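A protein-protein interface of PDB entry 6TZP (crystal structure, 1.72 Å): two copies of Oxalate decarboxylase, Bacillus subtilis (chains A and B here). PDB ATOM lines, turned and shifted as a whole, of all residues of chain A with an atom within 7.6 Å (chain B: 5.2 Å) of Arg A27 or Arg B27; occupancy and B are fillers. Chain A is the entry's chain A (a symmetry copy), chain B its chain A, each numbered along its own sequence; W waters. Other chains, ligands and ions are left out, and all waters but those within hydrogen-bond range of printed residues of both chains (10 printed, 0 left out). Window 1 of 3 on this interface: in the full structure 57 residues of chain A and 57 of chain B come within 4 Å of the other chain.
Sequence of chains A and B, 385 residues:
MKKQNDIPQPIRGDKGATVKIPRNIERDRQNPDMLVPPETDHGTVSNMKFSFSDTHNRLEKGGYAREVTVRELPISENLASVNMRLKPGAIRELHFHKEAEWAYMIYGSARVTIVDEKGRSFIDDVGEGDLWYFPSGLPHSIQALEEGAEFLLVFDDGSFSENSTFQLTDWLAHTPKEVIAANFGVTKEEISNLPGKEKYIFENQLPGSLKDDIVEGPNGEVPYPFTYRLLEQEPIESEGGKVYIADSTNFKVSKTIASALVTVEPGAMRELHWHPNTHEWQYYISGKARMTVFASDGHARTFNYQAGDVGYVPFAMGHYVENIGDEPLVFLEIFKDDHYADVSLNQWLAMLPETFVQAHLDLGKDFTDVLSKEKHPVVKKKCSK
The backbone carbonyl oxygen of Asn B24 sits at hydrogen-bond distance from the side-chain hydroxyl of Ser A53, at 3.5 Å. The guanidinium group (NH1) of Arg B27 is in salt-bridge range of the side-chain carboxylate (OD2) of Asp A54 (2.9 Å). The side-chain amide oxygen (OE1) of Gln A30 lies within hydrogen-bond range of the guanidinium group (NE) of Arg B27 (2.9 Å). The side-chain amide nitrogen (NE2) of Gln B30 is in hydrogen-bond range of the side-chain carboxylate (OE1) of Glu A26 (3.4 Å). The side-chain carboxylate of Asp B28 is in hydrogen-bond range of the side-chain hydroxyl of Ser A53 (2.8 Å). The side-chain carboxylate of Glu B26 is in hydrogen-bond range of the side-chain amide nitrogen of Gln A30, at 3.4 Å. NE2 of Gln B30 lies within hydrogen-bond range of OD1 of Asn A24, 2.9 Å away. ND2 of Asn B31 lies within hydrogen-bond range of O of Ser A53, 2.9 Å away. The side-chain hydroxyl of Ser B53 is in hydrogen-bond range of the backbone carbonyl oxygen of Asn A24, at 3.5 Å. OD2 of Asp B54 lies within salt-bridge range of NH1 of Arg A27, 2.9 Å away. The side-chain amide oxygen (OE1) of Gln B30 is in hydrogen-bond range of the guanidinium group (NE) of Arg A27, 2.9 Å away.
The side-chain amino group (NZ) of Lys A49 lies within hydrogen-bond range of the backbone carbonyl oxygen (O) of Asn A304 (2.7 Å). OD1 of Asp A54 is in salt-bridge range of NH2 of Arg A27 (2.8 Å).
Printed residues of chain B within 4 Å of Asn A24: Gln B30 (2.9 Å) and Ser B53 (3.5 Å). Arg A27 touches six residues of chain B. Asn A304 touches none of the printed residues of chain B. Of the printed residues of chain A, Asn B24 touches Gln A30, Ser A53 and Gln A306. Of chain A, only Arg A27 (3.2 Å), Gln A30 (2.9 Å), Asn A31 (3.8 Å), Ser A51 (3.8 Å), Ser A53 (3.6 Å) and Asp A54 (2.9 Å) come within 4 Å of Arg B27. The nearest residue of chain A that does not touch Arg B27 is Lys A49 (4.04 Å).
Along chain A the printed residues that touch a printed residue of chain B span positions 24 to 306. Of the 12 printed residues of chain B, 10 touch a printed residue of chain A. Among the printed residues, Asp or Glu carboxylates within 4 Å of a Lys or Arg side-chain nitrogen of the other chain: Arg A27 with Asp B54 and Asp A54 with Arg B27.
Arg A27 touches Ser B53, and with the chains exchanged Ser A53 touches Arg B27. Positions printed for both chains: 24, 25, 26, 27, 28, 29, 30, 31, 49, 51, 53 and 54.
Water W2 bridges the side-chain hydroxyl (OG) of Ser A53 (2.7 Å) and the backbone NH (N) of Asn B24 (2.9 Å).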
ATOM      1  N   PRO A   8       8.873   4.030  35.140  1.00  0.00           N
ATOM      2  CA  PRO A   8       9.798   2.989  34.673  1.00  0.00           C
ATOM      3  C   PRO A   8      11.167   3.565  34.357  1.00  0.00           C
ATOM      4  O   PRO A   8      11.309   4.741  34.007  1.00  0.00           O
ATOM      5  CB  PRO A   8       9.121   2.452  33.410  1.00  0.00           C
ATOM      6  CG  PRO A   8       8.318   3.632  32.895  1.00  0.00           C
ATOM      7  CD  PRO A   8       7.876   4.404  34.119  1.00  0.00           C
ATOM      8  N   ARG A  23      11.747  13.561  29.400  1.00  0.00           N
ATOM      9  CA  ARG A  23      11.432  12.293  28.757  1.00  0.00           C
ATOM     10  C   ARG A  23       9.927  12.166  28.554  1.00  0.00           C
ATOM     11  O   ARG A  23       9.133  12.941  29.097  1.00  0.00           O
ATOM     12  CB  ARG A  23      11.944  11.113  29.592  1.00  0.00           C
ATOM     13  CG  ARG A  23      11.314  11.063  30.974  1.00  0.00           C
ATOM     14  CD  ARG A  23      11.961  10.030  31.889  1.00  0.00           C
ATOM     15  NE  ARG A  23      11.683   8.674  31.446  1.00  0.00           N
ATOM     16  CZ  ARG A  23      11.732   7.606  32.236  1.00  0.00           C
ATOM     17  NH1 ARG A  23      12.061   7.732  33.524  1.00  0.00           N
ATOM     18  NH2 ARG A  23      11.452   6.414  31.735  1.00  0.00           N
ATOM     19  N   ASN A  24       9.546  11.148  27.778  1.00  0.00           N
ATOM     20  CA  ASN A  24       8.152  10.829  27.470  1.00  0.00           C
ATOM     21  C   ASN A  24       7.740   9.598  28.281  1.00  0.00           C
ATOM     22  O   ASN A  24       7.845   8.461  27.817  1.00  0.00           O
ATOM     23  CB  ASN A  24       7.982  10.593  25.972  1.00  0.00           C
ATOM     24  CG  ASN A  24       6.543  10.675  25.534  1.00  0.00           C
ATOM     25  OD1 ASN A  24       5.645  10.223  26.237  1.00  0.00           O
ATOM     26  ND2 ASN A  24       6.315  11.267  24.359  1.00  0.00           N
ATOM     27  N   ILE A  25       7.237   9.835  29.494  1.00  0.00           N
ATOM     28  CA  ILE A  25       6.917   8.723  30.387  1.00  0.00           C
ATOM     29  C   ILE A  25       5.760   7.901  29.840  1.00  0.00           C
ATOM     30  O   ILE A  25       5.747   6.669  29.968  1.00  0.00           O
ATOM     31  CB  ILE A  25       6.617   9.244  31.805  1.00  0.00           C
ATOM     32  CG1 ILE A  25       7.843   9.958  32.366  1.00  0.00           C
ATOM     33  CG2 ILE A  25       6.222   8.088  32.720  1.00  0.00           C
ATOM     34  CD1 ILE A  25       8.721   9.079  33.231  1.00  0.00           C
ATOM     35  N   GLU A  26       4.772   8.555  29.222  1.00  0.00           N
ATOM     36  CA  GLU A  26       3.631   7.813  28.686  1.00  0.00           C
ATOM     37  C   GLU A  26       4.056   6.839  27.595  1.00  0.00           C
ATOM     38  O   GLU A  26       3.586   5.695  27.562  1.00  0.00           O
ATOM     39  CB  GLU A  26       2.571   8.772  28.144  1.00  0.00           C
ATOM     40  CG  GLU A  26       1.881   9.617  29.207  1.00  0.00           C
ATOM     41  CD  GLU A  26       2.623  10.908  29.515  1.00  0.00           C
ATOM     42  OE1 GLU A  26       3.706  11.155  28.924  1.00  0.00           O
ATOM     43  OE2 GLU A  26       2.112  11.682  30.354  1.00  0.00           O
ATOM     44  N   ARG A  27       4.918   7.275  26.670  1.00  0.00           N
ATOM     45  CA  ARG A  27       5.391   6.349  25.644  1.00  0.00           C
ATOM     46  C   ARG A  27       6.277   5.271  26.250  1.00  0.00           C
ATOM     47  O   ARG A  27       6.227   4.114  25.824  1.00  0.00           O
ATOM     48  CB  ARG A  27       6.129   7.103  24.527  1.00  0.00           C
ATOM     49  CG  ARG A  27       5.177   7.715  23.504  1.00  0.00           C
ATOM     50  CD  ARG A  27       5.876   8.536  22.416  1.00  0.00           C
ATOM     51  NE  ARG A  27       4.909   9.461  21.818  1.00  0.00           N
ATOM     52  CZ  ARG A  27       4.580   9.495  20.529  1.00  0.00           C
ATOM     53  NH1 ARG A  27       5.159   8.677  19.662  1.00  0.00           N
ATOM     54  NH2 ARG A  27       3.676  10.367  20.107  1.00  0.00           N
ATOM     55  N   ASP A  28       7.099   5.624  27.248  1.00  0.00           N
ATOM     56  CA  ASP A  28       7.923   4.612  27.904  1.00  0.00           C
ATOM     57  C   ASP A  28       7.058   3.523  28.525  1.00  0.00           C
ATOM     58  O   ASP A  28       7.416   2.338  28.483  1.00  0.00           O
ATOM     59  CB  ASP A  28       8.817   5.253  28.975  1.00  0.00           C
ATOM     60  CG  ASP A  28       9.974   6.036  28.380  1.00  0.00           C
ATOM     61  OD1 ASP A  28      10.227   5.904  27.168  1.00  0.00           O
ATOM     62  OD2 ASP A  28      10.641   6.788  29.125  1.00  0.00           O
ATOM     63  N   ARG A  29       5.921   3.909  29.120  1.00  0.00           N
ATOM     64  CA  ARG A  29       5.032   2.922  29.731  1.00  0.00           C
ATOM     65  C   ARG A  29       4.411   2.010  28.685  1.00  0.00           C
ATOM     66  O   ARG A  29       4.126   0.843  28.978  1.00  0.00           O
ATOM     67  CB  ARG A  29       3.932   3.608  30.540  1.00  0.00           C
ATOM     68  CG  ARG A  29       4.369   4.147  31.898  1.00  0.00           C
ATOM     69  CD  ARG A  29       3.207   4.915  32.549  1.00  0.00           C
ATOM     70  NE  ARG A  29       3.620   5.666  33.733  1.00  0.00           N
ATOM     71  CZ  ARG A  29       3.211   6.900  34.020  1.00  0.00           C
ATOM     72  NH1 ARG A  29       2.375   7.544  33.204  1.00  0.00           N
ATOM     73  NH2 ARG A  29       3.646   7.499  35.121  1.00  0.00           N
ATOM     74  N   GLN A  30       4.195   2.522  27.469  1.00  0.00           N
ATOM     75  CA  GLN A  30       3.663   1.711  26.379  1.00  0.00           C
ATOM     76  C   GLN A  30       4.693   0.752  25.797  1.00  0.00           C
ATOM     77  O   GLN A  30       4.304  -0.244  25.168  1.00  0.00           O
ATOM     78  CB  GLN A  30       3.112   2.608  25.266  1.00  0.00           C
ATOM     79  CG  GLN A  30       1.922   3.459  25.718  1.00  0.00           C
ATOM     80  CD  GLN A  30       1.170   4.121  24.571  1.00  0.00           C
ATOM     81  OE1 GLN A  30       1.649   4.175  23.443  1.00  0.00           O
ATOM     82  NE2 GLN A  30      -0.024   4.639  24.868  1.00  0.00           N
ATOM     83  N   ASN A  31       5.985   1.010  26.011  1.00  0.00           N
ATOM     84  CA  ASN A  31       7.075   0.275  25.368  1.00  0.00           C
ATOM     85  C   ASN A  31       8.002  -0.373  26.393  1.00  0.00           C
ATOM     86  O   ASN A  31       9.220  -0.159  26.350  1.00  0.00           O
ATOM     87  CB  ASN A  31       7.872   1.216  24.461  1.00  0.00           C
ATOM     88  CG  ASN A  31       7.038   1.789  23.334  1.00  0.00           C
ATOM     89  OD1 ASN A  31       6.042   1.196  22.927  1.00  0.00           O
ATOM     90  ND2 ASN A  31       7.464   2.937  22.799  1.00  0.00           N
ATOM     91  N   PRO A  32       7.475  -1.197  27.311  1.00  0.00           N
ATOM     92  CA  PRO A  32       8.351  -1.735  28.369  1.00  0.00           C
ATOM     93  C   PRO A  32       9.498  -2.583  27.839  1.00  0.00           C
ATOM     94  O   PRO A  32      10.580  -2.597  28.444  1.00  0.00           O
ATOM     95  CB  PRO A  32       7.394  -2.566  29.236  1.00  0.00           C
ATOM     96  CG  PRO A  32       6.267  -2.935  28.308  1.00  0.00           C
ATOM     97  CD  PRO A  32       6.105  -1.739  27.410  1.00  0.00           C
ATOM     98  N   MET A  34      11.060  -2.151  25.061  1.00  0.00           N
ATOM     99  CA  MET A  34      11.992  -1.309  24.332  1.00  0.00           C
ATOM    100  C   MET A  34      12.818  -0.435  25.260  1.00  0.00           C
ATOM    101  O   MET A  34      14.033  -0.333  25.076  1.00  0.00           O
ATOM    102  CB  MET A  34      11.221  -0.471  23.302  1.00  0.00           C
ATOM    103  CG  MET A  34      10.398  -1.395  22.402  1.00  0.00           C
ATOM    104  SD  MET A  34       9.347  -0.590  21.190  1.00  0.00           S
ATOM    105  CE  MET A  34      10.614  -0.055  20.036  1.00  0.00           C
ATOM    106  N   LEU A  35      12.197   0.134  26.302  1.00  0.00           N
ATOM    107  CA  LEU A  35      12.970   0.768  27.374  1.00  0.00           C
ATOM    108  C   LEU A  35      13.859  -0.246  28.090  1.00  0.00           C
ATOM    109  O   LEU A  35      15.009   0.057  28.446  1.00  0.00           O
ATOM    110  CB  LEU A  35      12.021   1.433  28.368  1.00  0.00           C
ATOM    111  CG  LEU A  35      12.680   2.342  29.412  1.00  0.00           C
ATOM    112  CD1 LEU A  35      13.099   3.650  28.756  1.00  0.00           C
ATOM    113  CD2 LEU A  35      11.726   2.601  30.572  1.00  0.00           C
ATOM    114  N   LYS A  49       7.690  -0.784  13.735  1.00  0.00           N
ATOM    115  CA  LYS A  49       6.533  -0.404  14.541  1.00  0.00           C
ATOM    116  C   LYS A  49       6.158   1.050  14.273  1.00  0.00           C
ATOM    117  O   LYS A  49       7.034   1.916  14.295  1.00  0.00           O
ATOM    118  CB  LYS A  49       6.865  -0.602  16.027  1.00  0.00           C
ATOM    119  CG  LYS A  49       6.035   0.170  17.023  1.00  0.00           C
ATOM    120  CD  LYS A  49       6.789   0.198  18.354  1.00  0.00           C
ATOM    121  CE  LYS A  49       6.140   1.142  19.350  1.00  0.00           C
ATOM    122  NZ  LYS A  49       4.833   0.635  19.791  1.00  0.00           N
ATOM    123  N   PHE A  50       4.874   1.320  14.020  1.00  0.00           N
ATOM    124  CA  PHE A  50       4.428   2.700  13.843  1.00  0.00           C
ATOM    125  C   PHE A  50       2.955   2.822  14.211  1.00  0.00           C
ATOM    126  O   PHE A  50       2.151   1.957  13.853  1.00  0.00           O
ATOM    127  CB  PHE A  50       4.641   3.197  12.400  1.00  0.00           C
ATOM    128  CG  PHE A  50       4.777   4.695  12.299  1.00  0.00           C
ATOM    129  CD1 PHE A  50       3.648   5.505  12.166  1.00  0.00           C
ATOM    130  CD2 PHE A  50       6.030   5.296  12.362  1.00  0.00           C
ATOM    131  CE1 PHE A  50       3.770   6.903  12.097  1.00  0.00           C
ATOM    132  CE2 PHE A  50       6.161   6.673  12.278  1.00  0.00           C
ATOM    133  CZ  PHE A  50       5.027   7.482  12.143  1.00  0.00           C
ATOM    134  N   SER A  51       2.592   3.921  14.884  1.00  0.00           N
ATOM    135  CA  SER A  51       1.212   4.139  15.322  1.00  0.00           C
ATOM    136  C   SER A  51       0.420   5.051  14.384  1.00  0.00           C
ATOM    137  O   SER A  51       0.883   6.141  14.038  1.00  0.00           O
ATOM    138  CB  SER A  51       1.190   4.758  16.718  1.00  0.00           C
ATOM    139  OG  SER A  51      -0.163   4.953  17.105  1.00  0.00           O
ATOM    140  N   PHE A  52      -0.821   4.653  14.060  1.00  0.00           N
ATOM    141  CA  PHE A  52      -1.706   5.573  13.338  1.00  0.00           C
ATOM    142  C   PHE A  52      -1.933   6.859  14.128  1.00  0.00           C
ATOM    143  O   PHE A  52      -2.190   7.916  13.531  1.00  0.00           O
ATOM    144  CB  PHE A  52      -3.064   4.912  13.041  1.00  0.00           C
ATOM    145  CG  PHE A  52      -3.104   4.098  11.763  1.00  0.00           C
ATOM    146  CD1 PHE A  52      -3.265   4.713  10.529  1.00  0.00           C
ATOM    147  CD2 PHE A  52      -3.020   2.712  11.806  1.00  0.00           C
ATOM    148  CE1 PHE A  52      -3.323   3.967   9.366  1.00  0.00           C
ATOM    149  CE2 PHE A  52      -3.072   1.949  10.636  1.00  0.00           C
ATOM    150  CZ  PHE A  52      -3.227   2.580   9.412  1.00  0.00           C
ATOM    151  N   SER A  53      -1.857   6.797  15.470  1.00  0.00           N
ATOM    152  CA  SER A  53      -2.025   8.012  16.268  1.00  0.00           C
ATOM    153  C   SER A  53      -0.914   9.017  16.024  1.00  0.00           C
ATOM    154  O   SER A  53      -1.068  10.193  16.376  1.00  0.00           O
ATOM    155  CB  SER A  53      -2.062   7.682  17.758  1.00  0.00           C
ATOM    156  OG  SER A  53      -3.273   7.045  18.086  1.00  0.00           O
ATOM    157  N   ASP A  54       0.204   8.580  15.447  1.00  0.00           N
ATOM    158  CA  ASP A  54       1.299   9.479  15.123  1.00  0.00           C
ATOM    159  C   ASP A  54       1.233   9.981  13.679  1.00  0.00           C
ATOM    160  O   ASP A  54       2.267  10.372  13.118  1.00  0.00           O
ATOM    161  CB  ASP A  54       2.637   8.783  15.399  1.00  0.00           C
ATOM    162  CG  ASP A  54       2.932   8.650  16.900  1.00  0.00           C
ATOM    163  OD1 ASP A  54       2.670   9.604  17.650  1.00  0.00           O
ATOM    164  OD2 ASP A  54       3.435   7.590  17.326  1.00  0.00           O
ATOM    165  N   ASN A 304       7.125  -3.492  21.068  1.00  0.00           N
ATOM    166  CA  ASN A 304       5.813  -3.498  21.708  1.00  0.00           C
ATOM    167  C   ASN A 304       4.767  -2.950  20.751  1.00  0.00           C
ATOM    168  O   ASN A 304       5.047  -2.022  19.984  1.00  0.00           O
ATOM    169  CB  ASN A 304       5.808  -2.651  22.986  1.00  0.00           C
ATOM    170  CG  ASN A 304       6.562  -3.309  24.111  1.00  0.00           C
ATOM    171  OD1 ASN A 304       7.620  -2.837  24.511  1.00  0.00           O
ATOM    172  ND2 ASN A 304       6.036  -4.424  24.614  1.00  0.00           N
ATOM    173  N   GLN A 306       0.259  -2.115  20.413  1.00  0.00           N
ATOM    174  CA  GLN A 306      -1.094  -2.101  20.954  1.00  0.00           C
ATOM    175  C   GLN A 306      -2.046  -1.570  19.889  1.00  0.00           C
ATOM    176  O   GLN A 306      -1.644  -1.271  18.760  1.00  0.00           O
ATOM    177  CB  GLN A 306      -1.171  -1.290  22.253  1.00  0.00           C
ATOM    178  CG  GLN A 306      -0.730   0.153  22.147  1.00  0.00           C
ATOM    179  CD  GLN A 306      -0.762   0.826  23.514  1.00  0.00           C
ATOM    180  OE1 GLN A 306       0.117   0.602  24.360  1.00  0.00           O
ATOM    181  NE2 GLN A 306      -1.807   1.606  23.756  1.00  0.00           N
ATOM    182  N   ALA A 307      -3.331  -1.484  20.250  1.00  0.00           N
ATOM    183  CA  ALA A 307      -4.358  -1.081  19.295  1.00  0.00           C
ATOM    184  C   ALA A 307      -3.933   0.171  18.542  1.00  0.00           C
ATOM    185  O   ALA A 307      -3.498   1.154  19.147  1.00  0.00           O
ATOM    186  CB  ALA A 307      -5.683  -0.832  20.020  1.00  0.00           C
ATOM    187  N   ASP A 309      -1.543   0.151  16.135  1.00  0.00           N
ATOM    188  CA  ASP A 309      -0.162   0.057  15.668  1.00  0.00           C
ATOM    189  C   ASP A 309      -0.049  -0.798  14.411  1.00  0.00           C
ATOM    190  O   ASP A 309      -0.757  -1.796  14.246  1.00  0.00           O
ATOM    191  CB  ASP A 309       0.759  -0.543  16.739  1.00  0.00           C
ATOM    192  CG  ASP A 309       1.092   0.437  17.853  1.00  0.00           C
ATOM    193  OD1 ASP A 309       0.912   1.654  17.655  1.00  0.00           O
ATOM    194  OD2 ASP A 309       1.558  -0.014  18.924  1.00  0.00           O
ATOM    195  N   ASN B  24      -5.358   4.531  20.569  1.00  0.00           N
ATOM    196  CA  ASN B  24      -4.302   4.935  21.496  1.00  0.00           C
ATOM    197  C   ASN B  24      -4.607   6.348  22.001  1.00  0.00           C
ATOM    198  O   ASN B  24      -4.151   7.343  21.435  1.00  0.00           O
ATOM    199  CB  ASN B  24      -2.941   4.871  20.808  1.00  0.00           C
ATOM    200  CG  ASN B  24      -1.798   4.863  21.789  1.00  0.00           C
ATOM    201  OD1 ASN B  24      -1.836   5.552  22.804  1.00  0.00           O
ATOM    202  ND2 ASN B  24      -0.768   4.068  21.491  1.00  0.00           N
ATOM    203  N   ILE B  25      -5.363   6.428  23.098  1.00  0.00           N
ATOM    204  CA  ILE B  25      -5.800   7.732  23.595  1.00  0.00           C
ATOM    205  C   ILE B  25      -4.618   8.548  24.097  1.00  0.00           C
ATOM    206  O   ILE B  25      -4.576   9.772  23.917  1.00  0.00           O
ATOM    207  CB  ILE B  25      -6.869   7.557  24.690  1.00  0.00           C
ATOM    208  CG1 ILE B  25      -8.088   6.841  24.116  1.00  0.00           C
ATOM    209  CG2 ILE B  25      -7.278   8.916  25.251  1.00  0.00           C
ATOM    210  CD1 ILE B  25      -9.186   7.776  23.654  1.00  0.00           C
ATOM    211  N   GLU B  26      -3.639   7.896  24.730  1.00  0.00           N
ATOM    212  CA  GLU B  26      -2.485   8.634  25.241  1.00  0.00           C
ATOM    213  C   GLU B  26      -1.703   9.304  24.118  1.00  0.00           C
ATOM    214  O   GLU B  26      -1.287  10.462  24.251  1.00  0.00           O
ATOM    215  CB  GLU B  26      -1.563   7.710  26.038  1.00  0.00           C
ATOM    216  CG  GLU B  26      -2.161   7.191  27.339  1.00  0.00           C
ATOM    217  CD  GLU B  26      -2.970   5.916  27.155  1.00  0.00           C
ATOM    218  OE1 GLU B  26      -3.103   5.430  26.002  1.00  0.00           O
ATOM    219  OE2 GLU B  26      -3.473   5.398  28.176  1.00  0.00           O
ATOM    220  N   ARG B  27      -1.459   8.588  23.015  1.00  0.00           N
ATOM    221  CA  ARG B  27      -0.764   9.219  21.895  1.00  0.00           C
ATOM    222  C   ARG B  27      -1.630  10.292  21.251  1.00  0.00           C
ATOM    223  O   ARG B  27      -1.117  11.332  20.830  1.00  0.00           O
ATOM    224  CB  ARG B  27      -0.329   8.169  20.861  1.00  0.00           C
ATOM    225  CG  ARG B  27       0.970   7.469  21.246  1.00  0.00           C
ATOM    226  CD  ARG B  27       1.394   6.365  20.273  1.00  0.00           C
ATOM    227  NE  ARG B  27       2.314   5.451  20.956  1.00  0.00           N
ATOM    228  CZ  ARG B  27       3.558   5.186  20.566  1.00  0.00           C
ATOM    229  NH1 ARG B  27       4.052   5.733  19.464  1.00  0.00           N
ATOM    230  NH2 ARG B  27       4.304   4.354  21.277  1.00  0.00           N
ATOM    231  N   ASP B  28      -2.946  10.064  21.164  1.00  0.00           N
ATOM    232  CA  ASP B  28      -3.827  11.091  20.610  1.00  0.00           C
ATOM    233  C   ASP B  28      -3.743  12.377  21.422  1.00  0.00           C
ATOM    234  O   ASP B  28      -3.769  13.478  20.856  1.00  0.00           O
ATOM    235  CB  ASP B  28      -5.277  10.590  20.561  1.00  0.00           C
ATOM    236  CG  ASP B  28      -5.509   9.573  19.458  1.00  0.00           C
ATOM    237  OD1 ASP B  28      -4.629   9.419  18.590  1.00  0.00           O
ATOM    238  OD2 ASP B  28      -6.578   8.922  19.450  1.00  0.00           O
ATOM    239  N   ARG B  29      -3.655  12.256  22.754  1.00  0.00           N
ATOM    240  CA  ARG B  29      -3.561  13.443  23.601  1.00  0.00           C
ATOM    241  C   ARG B  29      -2.250  14.181  23.381  1.00  0.00           C
ATOM    242  O   ARG B  29      -2.203  15.408  23.525  1.00  0.00           O
ATOM    243  CB  ARG B  29      -3.706  13.071  25.077  1.00  0.00           C
ATOM    244  CG  ARG B  29      -5.131  12.783  25.533  1.00  0.00           C
ATOM    245  CD  ARG B  29      -5.120  12.305  26.995  1.00  0.00           C
ATOM    246  NE  ARG B  29      -6.413  11.777  27.426  1.00  0.00           N
ATOM    247  CZ  ARG B  29      -6.567  10.684  28.172  1.00  0.00           C
ATOM    248  NH1 ARG B  29      -5.506   9.984  28.574  1.00  0.00           N
ATOM    249  NH2 ARG B  29      -7.786  10.283  28.509  1.00  0.00           N
ATOM    250  N   GLN B  30      -1.183  13.454  23.034  1.00  0.00           N
ATOM    251  CA  GLN B  30       0.104  14.074  22.738  1.00  0.00           C
ATOM    252  C   GLN B  30       0.131  14.767  21.382  1.00  0.00           C
ATOM    253  O   GLN B  30       0.978  15.646  21.169  1.00  0.00           O
ATOM    254  CB  GLN B  30       1.227  13.033  22.804  1.00  0.00           C
ATOM    255  CG  GLN B  30       1.408  12.437  24.203  1.00  0.00           C
ATOM    256  CD  GLN B  30       2.696  11.639  24.367  1.00  0.00           C
ATOM    257  OE1 GLN B  30       3.360  11.296  23.395  1.00  0.00           O
ATOM    258  NE2 GLN B  30       3.046  11.335  25.618  1.00  0.00           N
ATOM    259  N   ASN B  31      -0.786  14.414  20.477  1.00  0.00           N
ATOM    260  CA  ASN B  31      -0.767  14.868  19.087  1.00  0.00           C
ATOM    261  C   ASN B  31      -2.051  15.607  18.716  1.00  0.00           C
ATOM    262  O   ASN B  31      -2.709  15.251  17.730  1.00  0.00           O
ATOM    263  CB  ASN B  31      -0.561  13.674  18.153  1.00  0.00           C
ATOM    264  CG  ASN B  31       0.765  12.977  18.377  1.00  0.00           C
ATOM    265  OD1 ASN B  31       1.716  13.581  18.866  1.00  0.00           O
ATOM    266  ND2 ASN B  31       0.843  11.701  17.986  1.00  0.00           N
ATOM    267  N   LYS B  49       8.649  13.393  12.306  1.00  0.00           N
ATOM    268  CA  LYS B  49       8.574  13.324  13.763  1.00  0.00           C
ATOM    269  C   LYS B  49       8.836  11.900  14.239  1.00  0.00           C
ATOM    270  O   LYS B  49       8.238  10.963  13.706  1.00  0.00           O
ATOM    271  CB  LYS B  49       7.183  13.791  14.220  1.00  0.00           C
ATOM    272  CG  LYS B  49       6.727  13.344  15.587  1.00  0.00           C
ATOM    273  CD  LYS B  49       5.207  13.508  15.660  1.00  0.00           C
ATOM    274  CE  LYS B  49       4.630  12.874  16.913  1.00  0.00           C
ATOM    275  NZ  LYS B  49       5.040  13.608  18.119  1.00  0.00           N
ATOM    276  N   SER B  51       9.959   9.646  18.110  1.00  0.00           N
ATOM    277  CA  SER B  51      10.329   9.682  19.526  1.00  0.00           C
ATOM    278  C   SER B  51      11.437   8.691  19.885  1.00  0.00           C
ATOM    279  O   SER B  51      11.345   7.506  19.550  1.00  0.00           O
ATOM    280  CB  SER B  51       9.115   9.376  20.400  1.00  0.00           C
ATOM    281  OG  SER B  51       9.514   9.422  21.763  1.00  0.00           O
ATOM    282  N   SER B  53      11.588   7.482  22.701  1.00  0.00           N
ATOM    283  CA  SER B  53      10.881   6.488  23.509  1.00  0.00           C
ATOM    284  C   SER B  53      10.359   5.334  22.672  1.00  0.00           C
ATOM    285  O   SER B  53      10.018   4.283  23.230  1.00  0.00           O
ATOM    286  CB  SER B  53       9.705   7.124  24.245  1.00  0.00           C
ATOM    287  OG  SER B  53      10.171   7.950  25.286  1.00  0.00           O
ATOM    288  N   ASP B  54      10.273   5.510  21.356  1.00  0.00           N
ATOM    289  CA  ASP B  54       9.838   4.445  20.468  1.00  0.00           C
ATOM    290  C   ASP B  54      11.013   3.663  19.877  1.00  0.00           C
ATOM    291  O   ASP B  54      10.865   3.047  18.811  1.00  0.00           O
ATOM    292  CB  ASP B  54       8.954   5.026  19.358  1.00  0.00           C
ATOM    293  CG  ASP B  54       7.565   5.436  19.866  1.00  0.00           C
ATOM    294  OD1 ASP B  54       6.978   4.695  20.673  1.00  0.00           O
ATOM    295  OD2 ASP B  54       7.057   6.497  19.449  1.00  0.00           O
HETATM  296  O   HOH W   1      -1.336   2.748  18.840  1.00  0.00           O
HETATM  297  O   HOH W   2      -5.052   5.030  17.757  1.00  0.00           O
HETATM  298  O   HOH W   3      11.649  10.040  26.167  1.00  0.00           O
HETATM  299  O   HOH W   4       8.973  12.060  23.175  1.00  0.00           O
HETATM  300  O   HOH W   5      11.027   3.656  25.777  1.00  0.00           O
HETATM  301  O   HOH W   6       5.089  10.737  13.858  1.00  0.00           O
HETATM  302  O   HOH W   7       1.760   2.354  20.622  1.00  0.00           O
HETATM  303  O   HOH W   8       8.662   2.526  16.934  1.00  0.00           O
HETATM  304  O   HOH W   9       5.844  12.462  21.455  1.00  0.00           O
HETATM  305  O   HOH W  10      -3.660  11.220  16.734  1.00  0.00           O
